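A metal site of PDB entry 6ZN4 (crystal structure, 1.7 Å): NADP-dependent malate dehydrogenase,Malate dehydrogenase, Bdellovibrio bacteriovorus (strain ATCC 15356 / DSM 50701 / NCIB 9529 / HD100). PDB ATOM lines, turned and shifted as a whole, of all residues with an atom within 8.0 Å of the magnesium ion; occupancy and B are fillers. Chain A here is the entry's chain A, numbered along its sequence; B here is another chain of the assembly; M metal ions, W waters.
The magnesium ion is bound by OD1 of Asp 161 (2.0 Å), OE2 of Glu 160 (2.1 Å), OD1 of Asp 186 (2.1 Å), water W1 (2.2 Å), water W3 (2.2 Å) and water W2 (2.4 Å).
The side-chain carboxylate (OD2) of Asp 161 is in hydrogen-bond range of the backbone NH (N) of Leu 101 (3.1 Å). The backbone carbonyl oxygen (O) of Glu 160 is in hydrogen-bond range of the side-chain hydroxyl (OG) of Ser 95, 2.7 Å away. O of Asp 161 sits at hydrogen-bond distance from N of Ala 99 (3.1 Å). The side-chain carboxylate (OD2) of Asp 186 is in hydrogen-bond range of a ring nitrogen (NE2) of His 184, at 3.0 Å. OE1 of Glu 160 lies within salt-bridge range of NZ of Lys 118 (3.1 Å). OE1 of Glu 160 lies within hydrogen-bond range of ND2 of Asn 158 (3.2 Å). The backbone carbonyl oxygen (O) of Asp 161 sits at hydrogen-bond distance from the side-chain hydroxyl (OG) of Ser 95, 3.2 Å away.
Three residues have an atom within 4 Å of the magnesium ion: Glu 160, Asp 161 and Asp 186. The nearest printed residue that does not touch the magnesium ion is Tyr 63 of chain B (4.1 Å).
Water W1 lies within hydrogen-bond range of the side-chain hydroxyl (OH) of Tyr 63 of chain B and the side-chain carboxylate (OD2) of Asp 161.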
ATOM      1  N   SER A  95      25.183 -23.392  20.160  1.00  0.00           N
ATOM      2  CA  SER A  95      25.902 -22.933  21.352  1.00  0.00           C
ATOM      3  C   SER A  95      26.197 -24.098  22.282  1.00  0.00           C
ATOM      4  O   SER A  95      25.435 -25.064  22.304  1.00  0.00           O
ATOM      5  CB  SER A  95      25.074 -21.889  22.110  1.00  0.00           C
ATOM      6  OG  SER A  95      25.813 -21.368  23.227  1.00  0.00           O
ATOM      7  N   ALA A  99      29.190 -19.178  27.434  1.00  0.00           N
ATOM      8  CA  ALA A  99      29.198 -17.727  27.649  1.00  0.00           C
ATOM      9  C   ALA A  99      27.863 -17.122  27.248  1.00  0.00           C
ATOM     10  O   ALA A  99      27.765 -16.417  26.249  1.00  0.00           O
ATOM     11  CB  ALA A  99      30.325 -17.065  26.869  1.00  0.00           C
ATOM     12  N   VAL A 100      26.835 -17.393  28.040  1.00  0.00           N
ATOM     13  CA  VAL A 100      25.478 -16.982  27.713  1.00  0.00           C
ATOM     14  C   VAL A 100      25.259 -15.571  28.216  1.00  0.00           C
ATOM     15  O   VAL A 100      25.361 -15.321  29.425  1.00  0.00           O
ATOM     16  CB  VAL A 100      24.450 -17.933  28.341  1.00  0.00           C
ATOM     17  CG1 VAL A 100      23.040 -17.482  28.029  1.00  0.00           C
ATOM     18  CG2 VAL A 100      24.683 -19.346  27.843  1.00  0.00           C
ATOM     19  N   LEU A 101      24.992 -14.664  27.280  1.00  0.00           N
ATOM     20  CA  LEU A 101      24.800 -13.238  27.580  1.00  0.00           C
ATOM     21  C   LEU A 101      25.909 -12.773  28.529  1.00  0.00           C
ATOM     22  O   LEU A 101      27.078 -12.970  28.227  1.00  0.00           O
ATOM     23  CB  LEU A 101      23.403 -12.989  28.181  1.00  0.00           C
ATOM     24  CG  LEU A 101      22.250 -13.216  27.191  1.00  0.00           C
ATOM     25  CD1 LEU A 101      20.885 -13.069  27.853  1.00  0.00           C
ATOM     26  CD2 LEU A 101      22.351 -12.302  25.967  1.00  0.00           C
ATOM     27  N   GLY A 102      25.540 -12.212  29.670  1.00  0.00           N
ATOM     28  CA  GLY A 102      26.501 -11.871  30.709  1.00  0.00           C
ATOM     29  C   GLY A 102      26.467 -12.829  31.879  1.00  0.00           C
ATOM     30  O   GLY A 102      26.978 -12.528  32.958  1.00  0.00           O
ATOM     31  N   VAL A 114      17.976 -18.410  25.187  1.00  0.00           N
ATOM     32  CA  VAL A 114      18.691 -17.388  24.444  1.00  0.00           C
ATOM     33  C   VAL A 114      18.797 -17.786  22.977  1.00  0.00           C
ATOM     34  O   VAL A 114      18.632 -16.943  22.091  1.00  0.00           O
ATOM     35  CB  VAL A 114      20.104 -17.132  25.054  1.00  0.00           C
ATOM     36  CG1 VAL A 114      20.975 -16.360  24.099  1.00  0.00           C
ATOM     37  CG2 VAL A 114      19.988 -16.347  26.353  1.00  0.00           C
ATOM     38  N   MET A 115      19.065 -19.060  22.708  1.00  0.00           N
ATOM     39  CA  MET A 115      19.234 -19.504  21.321  1.00  0.00           C
ATOM     40  C   MET A 115      17.881 -19.473  20.587  1.00  0.00           C
ATOM     41  O   MET A 115      17.807 -19.075  19.428  1.00  0.00           O
ATOM     42  CB  MET A 115      19.869 -20.902  21.251  1.00  0.00           C
ATOM     43  CG  MET A 115      21.212 -21.063  21.988  1.00  0.00           C
ATOM     44  SD  MET A 115      22.294 -19.652  21.740  1.00  0.00           S
ATOM     45  CE  MET A 115      22.890 -19.379  23.422  1.00  0.00           C
ATOM     46  N   LYS A 118      17.492 -15.832  19.813  1.00  0.00           N
ATOM     47  CA  LYS A 118      18.345 -15.411  18.697  1.00  0.00           C
ATOM     48  C   LYS A 118      17.671 -15.822  17.395  1.00  0.00           C
ATOM     49  O   LYS A 118      17.674 -15.082  16.404  1.00  0.00           O
ATOM     50  CB  LYS A 118      19.740 -16.044  18.791  1.00  0.00           C
ATOM     51  CG  LYS A 118      20.713 -15.567  17.739  1.00  0.00           C
ATOM     52  CD  LYS A 118      21.289 -14.206  18.090  1.00  0.00           C
ATOM     53  CE  LYS A 118      22.474 -13.863  17.201  1.00  0.00           C
ATOM     54  NZ  LYS A 118      23.282 -12.764  17.803  1.00  0.00           N
ATOM     55  N   ASN A 158      25.286 -20.048  12.670  1.00  0.00           N
ATOM     56  CA  ASN A 158      25.582 -18.925  13.553  1.00  0.00           C
ATOM     57  C   ASN A 158      25.989 -19.483  14.926  1.00  0.00           C
ATOM     58  O   ASN A 158      25.140 -19.986  15.685  1.00  0.00           O
ATOM     59  CB  ASN A 158      24.363 -18.000  13.711  1.00  0.00           C
ATOM     60  CG  ASN A 158      24.652 -16.795  14.598  1.00  0.00           C
ATOM     61  OD1 ASN A 158      25.172 -15.776  14.149  1.00  0.00           O
ATOM     62  ND2 ASN A 158      24.297 -16.906  15.879  1.00  0.00           N
ATOM     63  N   LEU A 159      27.286 -19.462  15.199  1.00  0.00           N
ATOM     64  CA  LEU A 159      27.789 -19.844  16.517  1.00  0.00           C
ATOM     65  C   LEU A 159      27.427 -18.747  17.495  1.00  0.00           C
ATOM     66  O   LEU A 159      27.432 -17.564  17.131  1.00  0.00           O
ATOM     67  CB  LEU A 159      29.307 -20.069  16.480  1.00  0.00           C
ATOM     68  CG  LEU A 159      29.761 -21.206  15.568  1.00  0.00           C
ATOM     69  CD1 LEU A 159      31.291 -21.155  15.429  1.00  0.00           C
ATOM     70  CD2 LEU A 159      29.330 -22.544  16.158  1.00  0.00           C
ATOM     71  N   GLU A 160      27.058 -19.103  18.724  1.00  0.00           N
ATOM     72  CA  GLU A 160      26.624 -18.097  19.680  1.00  0.00           C
ATOM     73  C   GLU A 160      26.996 -18.495  21.083  1.00  0.00           C
ATOM     74  O   GLU A 160      26.885 -19.662  21.454  1.00  0.00           O
ATOM     75  CB  GLU A 160      25.110 -17.891  19.593  1.00  0.00           C
ATOM     76  CG  GLU A 160      24.576 -16.728  20.400  1.00  0.00           C
ATOM     77  CD  GLU A 160      24.847 -15.369  19.754  1.00  0.00           C
ATOM     78  OE1 GLU A 160      24.989 -15.293  18.509  1.00  0.00           O
ATOM     79  OE2 GLU A 160      24.931 -14.374  20.505  1.00  0.00           O
ATOM     80  N   ASP A 161      27.462 -17.517  21.860  1.00  0.00           N
ATOM     81  CA  ASP A 161      27.601 -17.683  23.324  1.00  0.00           C
ATOM     82  C   ASP A 161      28.488 -18.859  23.712  1.00  0.00           C
ATOM     83  O   ASP A 161      28.148 -19.689  24.553  1.00  0.00           O
ATOM     84  CB  ASP A 161      26.188 -17.774  23.950  1.00  0.00           C
ATOM     85  CG  ASP A 161      25.499 -16.411  23.968  1.00  0.00           C
ATOM     86  OD1 ASP A 161      25.999 -15.485  23.283  1.00  0.00           O
ATOM     87  OD2 ASP A 161      24.467 -16.242  24.657  1.00  0.00           O
ATOM     88  N   ILE A 162      29.660 -18.843  23.080  1.00  0.00           N
ATOM     89  CA  ILE A 162      30.752 -19.754  23.350  1.00  0.00           C
ATOM     90  C   ILE A 162      31.875 -18.909  23.908  1.00  0.00           C
ATOM     91  O   ILE A 162      32.226 -17.884  23.319  1.00  0.00           O
ATOM     92  CB  ILE A 162      31.204 -20.467  22.089  1.00  0.00           C
ATOM     93  CG1 ILE A 162      30.032 -21.275  21.511  1.00  0.00           C
ATOM     94  CG2 ILE A 162      32.362 -21.417  22.372  1.00  0.00           C
ATOM     95  CD1 ILE A 162      30.372 -21.876  20.140  1.00  0.00           C
ATOM     96  N   HIS A 184      30.551 -16.566  14.017  1.00  0.00           N
ATOM     97  CA  HIS A 184      30.281 -16.399  15.438  1.00  0.00           C
ATOM     98  C   HIS A 184      29.908 -14.946  15.727  1.00  0.00           C
ATOM     99  O   HIS A 184      30.789 -14.083  15.802  1.00  0.00           O
ATOM    100  CB  HIS A 184      31.477 -16.824  16.298  1.00  0.00           C
ATOM    101  CG  HIS A 184      31.219 -16.746  17.779  1.00  0.00           C
ATOM    102  ND1 HIS A 184      32.213 -16.882  18.718  1.00  0.00           N
ATOM    103  CD2 HIS A 184      30.068 -16.559  18.471  1.00  0.00           C
ATOM    104  CE1 HIS A 184      31.700 -16.760  19.934  1.00  0.00           C
ATOM    105  NE2 HIS A 184      30.392 -16.568  19.814  1.00  0.00           N
ATOM    106  N   ASP A 185      28.614 -14.688  15.889  1.00  0.00           N
ATOM    107  CA  ASP A 185      28.158 -13.305  15.984  1.00  0.00           C
ATOM    108  C   ASP A 185      28.719 -12.537  17.200  1.00  0.00           C
ATOM    109  O   ASP A 185      28.923 -11.327  17.119  1.00  0.00           O
ATOM    110  CB  ASP A 185      26.626 -13.232  16.003  1.00  0.00           C
ATOM    111  CG  ASP A 185      26.111 -11.798  15.960  1.00  0.00           C
ATOM    112  OD1 ASP A 185      26.369 -11.107  14.956  1.00  0.00           O
ATOM    113  OD2 ASP A 185      25.481 -11.338  16.948  1.00  0.00           O
ATOM    114  N   ASP A 186      28.991 -13.211  18.315  1.00  0.00           N
ATOM    115  CA  ASP A 186      29.536 -12.475  19.461  1.00  0.00           C
ATOM    116  C   ASP A 186      30.912 -11.935  19.148  1.00  0.00           C
ATOM    117  O   ASP A 186      31.328 -10.920  19.716  1.00  0.00           O
ATOM    118  CB  ASP A 186      29.577 -13.370  20.695  1.00  0.00           C
ATOM    119  CG  ASP A 186      28.216 -13.952  21.034  1.00  0.00           C
ATOM    120  OD1 ASP A 186      27.423 -13.263  21.715  1.00  0.00           O
ATOM    121  OD2 ASP A 186      27.914 -15.069  20.576  1.00  0.00           O
ATOM    122  N   GLN A 187      31.609 -12.603  18.236  1.00  0.00           N
ATOM    123  CA  GLN A 187      32.944 -12.171  17.852  1.00  0.00           C
ATOM    124  C   GLN A 187      32.900 -10.984  16.923  1.00  0.00           C
ATOM    125  O   GLN A 187      33.729 -10.100  17.046  1.00  0.00           O
ATOM    126  CB  GLN A 187      33.713 -13.294  17.143  1.00  0.00           C
ATOM    127  CG  GLN A 187      34.381 -14.273  18.073  1.00  0.00           C
ATOM    128  CD  GLN A 187      35.267 -15.223  17.332  1.00  0.00           C
ATOM    129  OE1 GLN A 187      36.169 -14.817  16.602  1.00  0.00           O
ATOM    130  NE2 GLN A 187      35.023 -16.513  17.499  1.00  0.00           N
ATOM    131  N   ASN A 343      23.830  -5.619  17.691  1.00  0.00           N
ATOM    132  CA  ASN A 343      24.217  -6.667  16.745  1.00  0.00           C
ATOM    133  C   ASN A 343      23.145  -7.020  15.737  1.00  0.00           C
ATOM    134  O   ASN A 343      23.446  -7.566  14.684  1.00  0.00           O
ATOM    135  CB  ASN A 343      24.648  -7.947  17.464  1.00  0.00           C
ATOM    136  CG  ASN A 343      25.987  -7.806  18.151  1.00  0.00           C
ATOM    137  OD1 ASN A 343      26.492  -6.697  18.334  1.00  0.00           O
ATOM    138  ND2 ASN A 343      26.613  -8.926  18.467  1.00  0.00           N
ATOM    139  N   TYR B  63      14.222 -11.772  24.059  1.00  0.00           N
ATOM    140  CA  TYR B  63      15.679 -11.714  24.022  1.00  0.00           C
ATOM    141  C   TYR B  63      16.145 -10.803  25.175  1.00  0.00           C
ATOM    142  O   TYR B  63      15.432 -10.626  26.144  1.00  0.00           O
ATOM    143  CB  TYR B  63      16.184 -11.225  22.652  1.00  0.00           C
ATOM    144  CG  TYR B  63      17.615 -11.664  22.354  1.00  0.00           C
ATOM    145  CD1 TYR B  63      17.949 -13.016  22.297  1.00  0.00           C
ATOM    146  CD2 TYR B  63      18.615 -10.736  22.139  1.00  0.00           C
ATOM    147  CE1 TYR B  63      19.248 -13.433  22.041  1.00  0.00           C
ATOM    148  CE2 TYR B  63      19.917 -11.132  21.883  1.00  0.00           C
ATOM    149  CZ  TYR B  63      20.234 -12.471  21.833  1.00  0.00           C
ATOM    150  OH  TYR B  63      21.540 -12.868  21.586  1.00  0.00           O
HETATM  151 MG    MG M   1      25.471 -13.734  22.396  1.00  0.00          MG
HETATM  152  O   HOH W   1      23.466 -14.168  23.070  1.00  0.00           O
HETATM  153  O   HOH W   2      24.849 -11.583  21.538  1.00  0.00           O
HETATM  154  O   HOH W   3      26.161 -12.739  24.187  1.00  0.00           O
